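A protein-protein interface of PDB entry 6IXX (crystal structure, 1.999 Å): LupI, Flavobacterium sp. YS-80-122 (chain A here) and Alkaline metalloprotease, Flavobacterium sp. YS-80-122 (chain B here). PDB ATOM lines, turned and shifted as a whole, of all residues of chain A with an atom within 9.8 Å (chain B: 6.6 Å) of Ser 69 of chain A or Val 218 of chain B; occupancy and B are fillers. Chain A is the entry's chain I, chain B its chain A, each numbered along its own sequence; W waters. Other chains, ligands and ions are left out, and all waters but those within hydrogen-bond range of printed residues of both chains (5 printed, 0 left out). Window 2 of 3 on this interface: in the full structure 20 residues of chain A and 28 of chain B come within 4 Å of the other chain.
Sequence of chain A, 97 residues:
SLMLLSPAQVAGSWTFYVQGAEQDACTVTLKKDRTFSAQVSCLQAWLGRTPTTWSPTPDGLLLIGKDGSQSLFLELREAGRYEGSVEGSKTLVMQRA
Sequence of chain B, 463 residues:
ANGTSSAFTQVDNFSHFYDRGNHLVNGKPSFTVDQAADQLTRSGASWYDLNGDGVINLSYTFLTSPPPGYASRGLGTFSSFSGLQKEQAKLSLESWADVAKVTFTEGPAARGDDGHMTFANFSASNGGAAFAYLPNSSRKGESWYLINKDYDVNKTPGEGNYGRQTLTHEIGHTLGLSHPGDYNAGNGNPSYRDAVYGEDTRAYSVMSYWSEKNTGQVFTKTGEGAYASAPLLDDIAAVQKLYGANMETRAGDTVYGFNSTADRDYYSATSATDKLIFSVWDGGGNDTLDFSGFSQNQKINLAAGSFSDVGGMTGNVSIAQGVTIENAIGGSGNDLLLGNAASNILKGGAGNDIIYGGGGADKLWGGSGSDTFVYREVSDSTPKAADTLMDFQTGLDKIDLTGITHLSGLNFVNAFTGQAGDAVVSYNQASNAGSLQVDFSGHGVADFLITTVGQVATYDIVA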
ATOM      1  N   THR A  50      -8.062 -19.009  20.110  1.00  0.00           N
ATOM      2  CA  THR A  50      -6.823 -18.268  20.336  1.00  0.00           C
ATOM      3  C   THR A  50      -5.625 -19.046  19.796  1.00  0.00           C
ATOM      4  O   THR A  50      -5.471 -20.229  20.117  1.00  0.00           O
ATOM      5  CB  THR A  50      -6.628 -18.014  21.823  1.00  0.00           C
ATOM      6  OG1 THR A  50      -7.845 -17.501  22.367  1.00  0.00           O
ATOM      7  CG2 THR A  50      -5.503 -17.007  22.058  1.00  0.00           C
ATOM      8  N   PRO A  51      -4.752 -18.431  18.998  1.00  0.00           N
ATOM      9  CA  PRO A  51      -3.516 -19.116  18.606  1.00  0.00           C
ATOM     10  C   PRO A  51      -2.574 -19.275  19.787  1.00  0.00           C
ATOM     11  O   PRO A  51      -2.603 -18.507  20.749  1.00  0.00           O
ATOM     12  CB  PRO A  51      -2.911 -18.191  17.544  1.00  0.00           C
ATOM     13  CG  PRO A  51      -3.489 -16.853  17.830  1.00  0.00           C
ATOM     14  CD  PRO A  51      -4.864 -17.087  18.406  1.00  0.00           C
ATOM     15  N   THR A  52      -1.734 -20.292  19.702  1.00  0.00           N
ATOM     16  CA  THR A  52      -0.746 -20.574  20.731  1.00  0.00           C
ATOM     17  C   THR A  52       0.687 -20.493  20.227  1.00  0.00           C
ATOM     18  O   THR A  52       1.592 -20.206  21.020  1.00  0.00           O
ATOM     19  CB  THR A  52      -0.997 -21.968  21.334  1.00  0.00           C
ATOM     20  OG1 THR A  52      -1.122 -22.920  20.275  1.00  0.00           O
ATOM     21  CG2 THR A  52      -2.292 -21.982  22.152  1.00  0.00           C
ATOM     22  N   THR A  53       0.922 -20.751  18.940  1.00  0.00           N
ATOM     23  CA  THR A  53       2.214 -20.519  18.307  1.00  0.00           C
ATOM     24  C   THR A  53       1.996 -19.790  16.988  1.00  0.00           C
ATOM     25  O   THR A  53       0.870 -19.680  16.493  1.00  0.00           O
ATOM     26  CB  THR A  53       2.979 -21.824  18.042  1.00  0.00           C
ATOM     27  OG1 THR A  53       2.242 -22.626  17.107  1.00  0.00           O
ATOM     28  CG2 THR A  53       3.195 -22.619  19.333  1.00  0.00           C
ATOM     29  N   SER A  55       4.237 -19.248  12.992  1.00  0.00           N
ATOM     30  CA  SER A  55       5.331 -19.743  12.173  1.00  0.00           C
ATOM     31  C   SER A  55       5.436 -18.885  10.916  1.00  0.00           C
ATOM     32  O   SER A  55       4.444 -18.711  10.194  1.00  0.00           O
ATOM     33  CB  SER A  55       5.116 -21.217  11.817  1.00  0.00           C
ATOM     34  OG  SER A  55       6.195 -21.742  11.064  1.00  0.00           O
ATOM     35  N   LEU A  62       1.732 -17.875   9.715  1.00  0.00           N
ATOM     36  CA  LEU A  62       0.657 -18.715  10.222  1.00  0.00           C
ATOM     37  C   LEU A  62       0.519 -18.487  11.724  1.00  0.00           C
ATOM     38  O   LEU A  62       1.521 -18.438  12.440  1.00  0.00           O
ATOM     39  CB  LEU A  62       0.940 -20.193   9.929  1.00  0.00           C
ATOM     40  CG  LEU A  62       0.902 -20.597   8.452  1.00  0.00           C
ATOM     41  CD1 LEU A  62       1.766 -21.827   8.227  1.00  0.00           C
ATOM     42  CD2 LEU A  62      -0.528 -20.842   7.972  1.00  0.00           C
ATOM     43  N   LEU A  63      -0.713 -18.298  12.186  1.00  0.00           N
ATOM     44  CA  LEU A  63      -1.039 -18.327  13.607  1.00  0.00           C
ATOM     45  C   LEU A  63      -1.676 -19.686  13.860  1.00  0.00           C
ATOM     46  O   LEU A  63      -2.673 -20.029  13.220  1.00  0.00           O
ATOM     47  CB  LEU A  63      -1.989 -17.189  13.988  1.00  0.00           C
ATOM     48  CG  LEU A  63      -1.655 -15.774  13.496  1.00  0.00           C
ATOM     49  CD1 LEU A  63      -2.812 -14.833  13.732  1.00  0.00           C
ATOM     50  CD2 LEU A  63      -0.406 -15.230  14.153  1.00  0.00           C
ATOM     51  N   ILE A  64      -1.068 -20.488  14.729  1.00  0.00           N
ATOM     52  CA  ILE A  64      -1.410 -21.904  14.840  1.00  0.00           C
ATOM     53  C   ILE A  64      -2.086 -22.158  16.181  1.00  0.00           C
ATOM     54  O   ILE A  64      -1.606 -21.698  17.224  1.00  0.00           O
ATOM     55  CB  ILE A  64      -0.169 -22.788  14.647  1.00  0.00           C
ATOM     56  CG1 ILE A  64       0.457 -22.494  13.278  1.00  0.00           C
ATOM     57  CG2 ILE A  64      -0.544 -24.262  14.746  1.00  0.00           C
ATOM     58  CD1 ILE A  64       1.761 -23.223  13.016  1.00  0.00           C
ATOM     59  N   GLY A  65      -3.199 -22.887  16.151  1.00  0.00           N
ATOM     60  CA  GLY A  65      -4.015 -23.100  17.330  1.00  0.00           C
ATOM     61  C   GLY A  65      -3.390 -24.085  18.296  1.00  0.00           C
ATOM     62  O   GLY A  65      -2.310 -24.630  18.072  1.00  0.00           O
ATOM     63  N   LYS A  66      -4.102 -24.344  19.391  1.00  0.00           N
ATOM     64  CA  LYS A  66      -3.508 -25.159  20.448  1.00  0.00           C
ATOM     65  C   LYS A  66      -3.298 -26.611  20.042  1.00  0.00           C
ATOM     66  O   LYS A  66      -2.428 -27.274  20.619  1.00  0.00           O
ATOM     67  CB  LYS A  66      -4.349 -25.114  21.721  1.00  0.00           C
ATOM     68  CG  LYS A  66      -3.609 -25.671  22.923  1.00  0.00           C
ATOM     69  CD  LYS A  66      -4.523 -26.504  23.789  1.00  0.00           C
ATOM     70  CE  LYS A  66      -5.758 -25.724  24.151  1.00  0.00           C
ATOM     71  NZ  LYS A  66      -5.436 -24.356  24.647  1.00  0.00           N
ATOM     72  N   ASP A  67      -4.043 -27.134  19.061  1.00  0.00           N
ATOM     73  CA  ASP A  67      -3.774 -28.512  18.666  1.00  0.00           C
ATOM     74  C   ASP A  67      -2.501 -28.643  17.843  1.00  0.00           C
ATOM     75  O   ASP A  67      -2.178 -29.751  17.405  1.00  0.00           O
ATOM     76  CB  ASP A  67      -4.974 -29.131  17.918  1.00  0.00           C
ATOM     77  CG  ASP A  67      -5.311 -28.445  16.573  1.00  0.00           C
ATOM     78  OD1 ASP A  67      -4.494 -27.724  15.962  1.00  0.00           O
ATOM     79  OD2 ASP A  67      -6.437 -28.676  16.104  1.00  0.00           O
ATOM     80  N   GLY A  68      -1.773 -27.544  17.641  1.00  0.00           N
ATOM     81  CA  GLY A  68      -0.557 -27.538  16.858  1.00  0.00           C
ATOM     82  C   GLY A  68      -0.751 -27.617  15.363  1.00  0.00           C
ATOM     83  O   GLY A  68       0.245 -27.703  14.633  1.00  0.00           O
ATOM     84  N   SER A  69      -1.993 -27.585  14.870  1.00  0.00           N
ATOM     85  CA  SER A  69      -2.185 -27.765  13.436  1.00  0.00           C
ATOM     86  C   SER A  69      -3.129 -26.725  12.822  1.00  0.00           C
ATOM     87  O   SER A  69      -2.803 -26.142  11.783  1.00  0.00           O
ATOM     88  CB  SER A  69      -2.682 -29.182  13.153  1.00  0.00           C
ATOM     89  OG  SER A  69      -3.400 -29.224  11.948  1.00  0.00           O
ATOM     90  N   GLN A  70      -4.284 -26.473  13.444  1.00  0.00           N
ATOM     91  CA  GLN A  70      -5.243 -25.523  12.886  1.00  0.00           C
ATOM     92  C   GLN A  70      -4.646 -24.117  12.853  1.00  0.00           C
ATOM     93  O   GLN A  70      -3.931 -23.707  13.771  1.00  0.00           O
ATOM     94  CB  GLN A  70      -6.539 -25.545  13.707  1.00  0.00           C
ATOM     95  CG  GLN A  70      -6.346 -25.156  15.161  1.00  0.00           C
ATOM     96  CD  GLN A  70      -7.410 -25.700  16.100  1.00  0.00           C
ATOM     97  OE1 GLN A  70      -7.111 -26.024  17.256  1.00  0.00           O
ATOM     98  NE2 GLN A  70      -8.654 -25.781  15.629  1.00  0.00           N
ATOM     99  N   SER A  71      -4.948 -23.369  11.792  1.00  0.00           N
ATOM    100  CA  SER A  71      -4.192 -22.161  11.486  1.00  0.00           C
ATOM    101  C   SER A  71      -5.067 -21.090  10.850  1.00  0.00           C
ATOM    102  O   SER A  71      -6.090 -21.385  10.230  1.00  0.00           O
ATOM    103  CB  SER A  71      -3.037 -22.465  10.521  1.00  0.00           C
ATOM    104  OG  SER A  71      -3.565 -22.817   9.237  1.00  0.00           O
ATOM    105  N   LEU A  72      -4.639 -19.839  11.023  1.00  0.00           N
ATOM    106  CA  LEU A  72      -5.052 -18.708  10.204  1.00  0.00           C
ATOM    107  C   LEU A  72      -3.819 -18.213   9.458  1.00  0.00           C
ATOM    108  O   LEU A  72      -2.779 -17.980  10.074  1.00  0.00           O
ATOM    109  CB  LEU A  72      -5.629 -17.579  11.058  1.00  0.00           C
ATOM    110  CG  LEU A  72      -5.928 -16.282  10.300  1.00  0.00           C
ATOM    111  CD1 LEU A  72      -7.074 -16.501   9.320  1.00  0.00           C
ATOM    112  CD2 LEU A  72      -6.255 -15.147  11.247  1.00  0.00           C
ATOM    113  N   PHE A  73      -3.917 -18.090   8.140  1.00  0.00           N
ATOM    114  CA  PHE A  73      -2.818 -17.574   7.338  1.00  0.00           C
ATOM    115  C   PHE A  73      -3.007 -16.083   7.100  1.00  0.00           C
ATOM    116  O   PHE A  73      -4.127 -15.617   6.873  1.00  0.00           O
ATOM    117  CB  PHE A  73      -2.714 -18.289   5.986  1.00  0.00           C
ATOM    118  CG  PHE A  73      -1.624 -17.733   5.092  1.00  0.00           C
ATOM    119  CD1 PHE A  73      -0.288 -17.942   5.401  1.00  0.00           C
ATOM    120  CD2 PHE A  73      -1.937 -16.978   3.970  1.00  0.00           C
ATOM    121  CE1 PHE A  73       0.730 -17.422   4.592  1.00  0.00           C
ATOM    122  CE2 PHE A  73      -0.931 -16.456   3.155  1.00  0.00           C
ATOM    123  CZ  PHE A  73       0.407 -16.679   3.476  1.00  0.00           C
ATOM    124  N   GLU B 212       0.327 -23.038   0.811  1.00  0.00           N
ATOM    125  CA  GLU B 212      -0.720 -24.023   0.562  1.00  0.00           C
ATOM    126  C   GLU B 212      -1.999 -23.684   1.308  1.00  0.00           C
ATOM    127  O   GLU B 212      -3.090 -24.014   0.832  1.00  0.00           O
ATOM    128  CB  GLU B 212      -0.242 -25.425   0.953  1.00  0.00           C
ATOM    129  CG  GLU B 212      -0.120 -25.657   2.476  1.00  0.00           C
ATOM    130  CD  GLU B 212       1.099 -24.983   3.091  1.00  0.00           C
ATOM    131  OE1 GLU B 212       1.899 -24.396   2.328  1.00  0.00           O
ATOM    132  OE2 GLU B 212       1.260 -25.030   4.341  1.00  0.00           O
ATOM    133  N   LYS B 213      -1.895 -23.012   2.464  1.00  0.00           N
ATOM    134  CA  LYS B 213      -3.097 -22.686   3.228  1.00  0.00           C
ATOM    135  C   LYS B 213      -4.060 -21.821   2.431  1.00  0.00           C
ATOM    136  O   LYS B 213      -5.266 -21.850   2.704  1.00  0.00           O
ATOM    137  CB  LYS B 213      -2.731 -22.006   4.554  1.00  0.00           C
ATOM    138  CG  LYS B 213      -3.898 -21.892   5.540  1.00  0.00           C
ATOM    139  CD  LYS B 213      -4.398 -23.263   6.013  1.00  0.00           C
ATOM    140  CE  LYS B 213      -5.849 -23.186   6.507  1.00  0.00           C
ATOM    141  NZ  LYS B 213      -6.020 -22.332   7.734  1.00  0.00           N
ATOM    142  N   GLY B 216      -6.458 -24.091   1.254  1.00  0.00           N
ATOM    143  CA  GLY B 216      -7.102 -24.862   2.302  1.00  0.00           C
ATOM    144  C   GLY B 216      -6.259 -25.973   2.908  1.00  0.00           C
ATOM    145  O   GLY B 216      -6.604 -26.480   3.988  1.00  0.00           O
ATOM    146  N   GLN B 217      -5.169 -26.353   2.257  1.00  0.00           N
ATOM    147  CA  GLN B 217      -4.362 -27.463   2.739  1.00  0.00           C
ATOM    148  C   GLN B 217      -3.709 -27.124   4.076  1.00  0.00           C
ATOM    149  O   GLN B 217      -3.236 -26.004   4.295  1.00  0.00           O
ATOM    150  CB  GLN B 217      -3.303 -27.834   1.696  1.00  0.00           C
ATOM    151  CG  GLN B 217      -3.889 -28.590   0.484  1.00  0.00           C
ATOM    152  CD  GLN B 217      -4.405 -27.681  -0.633  1.00  0.00           C
ATOM    153  OE1 GLN B 217      -4.526 -26.468  -0.470  1.00  0.00           O
ATOM    154  NE2 GLN B 217      -4.697 -28.276  -1.780  1.00  0.00           N
ATOM    155  N   VAL B 218      -3.704 -28.098   4.979  1.00  0.00           N
ATOM    156  CA  VAL B 218      -3.100 -27.952   6.299  1.00  0.00           C
ATOM    157  C   VAL B 218      -1.814 -28.770   6.288  1.00  0.00           C
ATOM    158  O   VAL B 218      -1.846 -30.003   6.361  1.00  0.00           O
ATOM    159  CB  VAL B 218      -4.058 -28.398   7.410  1.00  0.00           C
ATOM    160  CG1 VAL B 218      -3.368 -28.362   8.773  1.00  0.00           C
ATOM    161  CG2 VAL B 218      -5.322 -27.531   7.415  1.00  0.00           C
ATOM    162  N   PHE B 219      -0.670 -28.101   6.168  1.00  0.00           N
ATOM    163  CA  PHE B 219       0.621 -28.770   6.286  1.00  0.00           C
ATOM    164  C   PHE B 219       1.260 -28.558   7.656  1.00  0.00           C
ATOM    165  O   PHE B 219       2.420 -28.946   7.865  1.00  0.00           O
ATOM    166  CB  PHE B 219       1.597 -28.287   5.214  1.00  0.00           C
ATOM    167  CG  PHE B 219       1.272 -28.727   3.811  1.00  0.00           C
ATOM    168  CD1 PHE B 219       0.124 -29.442   3.523  1.00  0.00           C
ATOM    169  CD2 PHE B 219       2.138 -28.391   2.768  1.00  0.00           C
ATOM    170  CE1 PHE B 219      -0.160 -29.824   2.212  1.00  0.00           C
ATOM    171  CE2 PHE B 219       1.860 -28.758   1.457  1.00  0.00           C
ATOM    172  CZ  PHE B 219       0.705 -29.480   1.179  1.00  0.00           C
ATOM    173  N   THR B 220       0.554 -27.922   8.580  1.00  0.00           N
ATOM    174  CA  THR B 220       1.096 -27.659   9.907  1.00  0.00           C
ATOM    175  C   THR B 220       0.807 -28.837  10.827  1.00  0.00           C
ATOM    176  O   THR B 220      -0.309 -29.371  10.848  1.00  0.00           O
ATOM    177  CB  THR B 220       0.507 -26.375  10.485  1.00  0.00           C
ATOM    178  OG1 THR B 220      -0.908 -26.385  10.290  1.00  0.00           O
ATOM    179  CG2 THR B 220       1.115 -25.160   9.792  1.00  0.00           C
ATOM    180  N   LYS B 221       1.822 -29.242  11.576  1.00  0.00           N
ATOM    181  CA  LYS B 221       1.690 -30.288  12.572  1.00  0.00           C
ATOM    182  C   LYS B 221       2.640 -29.929  13.701  1.00  0.00           C
ATOM    183  O   LYS B 221       3.752 -29.448  13.459  1.00  0.00           O
ATOM    184  CB  LYS B 221       2.015 -31.665  11.981  1.00  0.00           C
ATOM    185  CG  LYS B 221       1.545 -32.863  12.773  1.00  0.00           C
ATOM    186  CD  LYS B 221       1.594 -34.091  11.879  1.00  0.00           C
ATOM    187  CE  LYS B 221       1.677 -35.386  12.669  1.00  0.00           C
ATOM    188  NZ  LYS B 221       1.950 -36.544  11.746  1.00  0.00           N
ATOM    189  N   THR B 222       2.193 -30.177  14.926  1.00  0.00           N
ATOM    190  CA  THR B 222       2.950 -29.895  16.142  1.00  0.00           C
ATOM    191  C   THR B 222       3.625 -28.513  16.086  1.00  0.00           C
ATOM    192  O   THR B 222       4.803 -28.334  16.409  1.00  0.00           O
ATOM    193  CB  THR B 222       3.930 -31.053  16.463  1.00  0.00           C
ATOM    194  OG1 THR B 222       4.886 -30.646  17.440  1.00  0.00           O
ATOM    195  CG2 THR B 222       4.652 -31.662  15.239  1.00  0.00           C
ATOM    196  N   GLY B 223       2.835 -27.511  15.682  1.00  0.00           N
ATOM    197  CA  GLY B 223       3.181 -26.111  15.874  1.00  0.00           C
ATOM    198  C   GLY B 223       3.961 -25.443  14.762  1.00  0.00           C
ATOM    199  O   GLY B 223       4.379 -24.291  14.928  1.00  0.00           O
ATOM    200  N   GLU B 224       4.134 -26.104  13.620  1.00  0.00           N
ATOM    201  CA  GLU B 224       5.017 -25.609  12.573  1.00  0.00           C
ATOM    202  C   GLU B 224       4.639 -26.289  11.268  1.00  0.00           C
ATOM    203  O   GLU B 224       4.183 -27.434  11.269  1.00  0.00           O
ATOM    204  CB  GLU B 224       6.475 -25.907  12.927  1.00  0.00           C
ATOM    205  CG  GLU B 224       7.498 -25.163  12.121  1.00  0.00           C
ATOM    206  CD  GLU B 224       8.903 -25.513  12.551  1.00  0.00           C
ATOM    207  OE1 GLU B 224       9.062 -26.515  13.292  1.00  0.00           O
ATOM    208  OE2 GLU B 224       9.846 -24.792  12.154  1.00  0.00           O
ATOM    209  N   VAL B 310      -3.174 -37.106   4.848  1.00  0.00           N
ATOM    210  CA  VAL B 310      -2.323 -38.112   5.468  1.00  0.00           C
ATOM    211  C   VAL B 310      -1.702 -37.545   6.738  1.00  0.00           C
ATOM    212  O   VAL B 310      -1.273 -36.386   6.771  1.00  0.00           O
ATOM    213  CB  VAL B 310      -1.223 -38.575   4.489  1.00  0.00           C
ATOM    214  CG1 VAL B 310      -0.143 -39.371   5.217  1.00  0.00           C
ATOM    215  CG2 VAL B 310      -1.824 -39.379   3.344  1.00  0.00           C
ATOM    216  N   GLY B 312      -2.658 -36.623   9.729  1.00  0.00           N
ATOM    217  CA  GLY B 312      -3.222 -35.465  10.388  1.00  0.00           C
ATOM    218  C   GLY B 312      -3.143 -34.176   9.594  1.00  0.00           C
ATOM    219  O   GLY B 312      -3.641 -33.147  10.062  1.00  0.00           O
ATOM    220  N   MET B 313      -2.542 -34.202   8.412  1.00  0.00           N
ATOM    221  CA  MET B 313      -2.522 -33.069   7.498  1.00  0.00           C
ATOM    222  C   MET B 313      -3.548 -33.287   6.379  1.00  0.00           C
ATOM    223  O   MET B 313      -4.129 -34.370   6.251  1.00  0.00           O
ATOM    224  CB  MET B 313      -1.102 -32.879   6.950  1.00  0.00           C
ATOM    225  CG  MET B 313      -0.062 -32.534   8.035  1.00  0.00           C
ATOM    226  SD  MET B 313       1.612 -33.163   7.727  1.00  0.00           S
ATOM    227  CE  MET B 313       2.102 -32.170   6.298  1.00  0.00           C
ATOM    228  N   THR B 314      -3.801 -32.234   5.577  1.00  0.00           N
ATOM    229  CA  THR B 314      -4.766 -32.319   4.479  1.00  0.00           C
ATOM    230  C   THR B 314      -4.131 -31.896   3.162  1.00  0.00           C
ATOM    231  O   THR B 314      -3.378 -30.918   3.106  1.00  0.00           O
ATOM    232  CB  THR B 314      -6.007 -31.452   4.720  1.00  0.00           C
ATOM    233  OG1 THR B 314      -5.642 -30.069   4.657  1.00  0.00           O
ATOM    234  CG2 THR B 314      -6.647 -31.766   6.078  1.00  0.00           C
ATOM    235  N   GLY B 315      -4.452 -32.639   2.101  1.00  0.00           N
ATOM    236  CA  GLY B 315      -3.955 -32.328   0.777  1.00  0.00           C
ATOM    237  C   GLY B 315      -2.458 -32.450   0.596  1.00  0.00           C
ATOM    238  O   GLY B 315      -1.904 -31.818  -0.309  1.00  0.00           O
ATOM    239  N   ASN B 316      -1.790 -33.260   1.421  1.00  0.00           N
ATOM    240  CA  ASN B 316      -0.333 -33.287   1.507  1.00  0.00           C
ATOM    241  C   ASN B 316       0.297 -34.447   0.746  1.00  0.00           C
ATOM    242  O   ASN B 316       1.518 -34.451   0.546  1.00  0.00           O
ATOM    243  CB  ASN B 316       0.099 -33.344   2.984  1.00  0.00           C
ATOM    244  CG  ASN B 316      -0.552 -34.495   3.737  1.00  0.00           C
ATOM    245  OD1 ASN B 316      -1.755 -34.740   3.599  1.00  0.00           O
ATOM    246  ND2 ASN B 316       0.242 -35.206   4.540  1.00  0.00           N
HETATM  247  O   HOH W   1      -1.849 -24.665   8.199  1.00  0.00           O
HETATM  248  O   HOH W   2      -6.125 -19.230   6.930  1.00  0.00           O
HETATM  249  O   HOH W   3      -7.022 -24.607  10.004  1.00  0.00           O
HETATM  250  O   HOH W   4      -0.358 -30.850  15.715  1.00  0.00           O
HETATM  251  O   HOH W   5       8.236 -22.099  12.385  1.00  0.00           O
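Ser 69 of chain A touches two residues of chain B.
Val 218 of chain B touches one residue of chain A.
No residue of chain A comes within 4 Å of Met 313 of chain B.
Thr 314 of chain B touches none of the printed residues of chain A.
Of the printed residues of chain B, Ser 55 of chain A touches Glu 224 (3.8 Å).
Printed residues of chain B within 4 Å of Phe 73 of chain A: Lys 213.
Of the printed residues of chain B, Ile 64 of chain A touches Thr 220 (3.8 Å), Gly 223 (3.4 Å) and Glu 224 (3.8 Å).
Printed residues of chain A within 4 Å of Thr 222 of chain B: Gly 68.
NZ of Lys 213 of chain B is in hydrogen-bond range of O of Ser 71 of chain A (2.7 Å).
The backbone carbonyl oxygen (O) of Ser 69 of chain A is in hydrogen-bond range of the side-chain hydroxyl (OG1) of Thr 220 of chain B (2.4 Å).
N of Thr 222 of chain B lies within hydrogen-bond range of O of Gly 68 of chain A (3.2 Å).
The backbone carbonyl oxygen (O) of Gly 223 of chain B sits at hydrogen-bond distance from the side-chain hydroxyl (OG1) of Thr 53 of chain A (3.5 Å).
N of Gly 223 of chain B lies within hydrogen-bond range of O of Gly 68 of chain A (2.8 Å).
The backbone NH (N) of Val 218 of chain B lies within hydrogen-bond range of the side-chain hydroxyl (OG1) of Thr 314 of chain B.
The backbone carbonyl oxygen (O) of Ile 64 of chain A sits at hydrogen-bond distance from the backbone NH (N) of Thr 52 of chain A, 2.9 Å away.
O of Thr 53 of chain A sits at hydrogen-bond distance from N of Ile 64 of chain A.
The backbone carbonyl oxygen of Ser 55 of chain A is in hydrogen-bond range of the backbone NH of Leu 62 of chain A, 2.9 Å away.
The backbone NH (N) of Ser 69 of chain A is in hydrogen-bond range of the side-chain carboxylate (OD1) of Asp 67 of chain A (2.7 Å).
Water W5 bridges the side-chain hydroxyl of Ser 55 of chain A (2.5 Å) and the side-chain carboxylate of Glu 224 of chain B (3.1 Å).
Water W4 lies within hydrogen-bond range of the backbone carbonyl oxygen (O) of Asp 67 of chain A (2.7 Å), the backbone NH (N) of Thr 222 of chain B (2.8 Å) and the backbone carbonyl oxygen (O) of Gly 68 of chain A (3.4 Å).
Water W1 bridges OG of Ser 71 of chain A (2.7 Å) and OG1 of Thr 220 of chain B (2.9 Å).
Water W2 lies within hydrogen-bond range of N of Phe 73 of chain A (2.8 Å) and NZ of Lys 213 of chain B (3.2 Å).
Water W3 lies within hydrogen-bond range of N of Ser 71 of chain A (3.0 Å) and NZ of Lys 213 of chain B (3.4 Å).
Among the printed residues, merely in contact across the chains: Ser 55 of chain A with Glu 224 of chain B (3.8 Å), Leu 62 of chain A with Thr 220 of chain B (3.7 Å), Ile 64 of chain A with Thr 220 of chain B (3.8 Å), Ile 64 of chain A with Gly 223 of chain B (3.4 Å), Ile 64 of chain A with Glu 224 of chain B (3.8 Å), Gly 68 of chain A with Lys 221 of chain B (3.4 Å), Ser 69 of chain A with Val 218 of chain B (3.3 Å) and Phe 73 of chain A with Lys 213 of chain B (3.8 Å).
Hydrophobic or aromatic side chains of chain B that line the printed part of chain A: Val 218.
Among the printed residues, no Asp or Glu carboxylate lies within 4 Å of a Lys or Arg side-chain nitrogen of the other chain.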
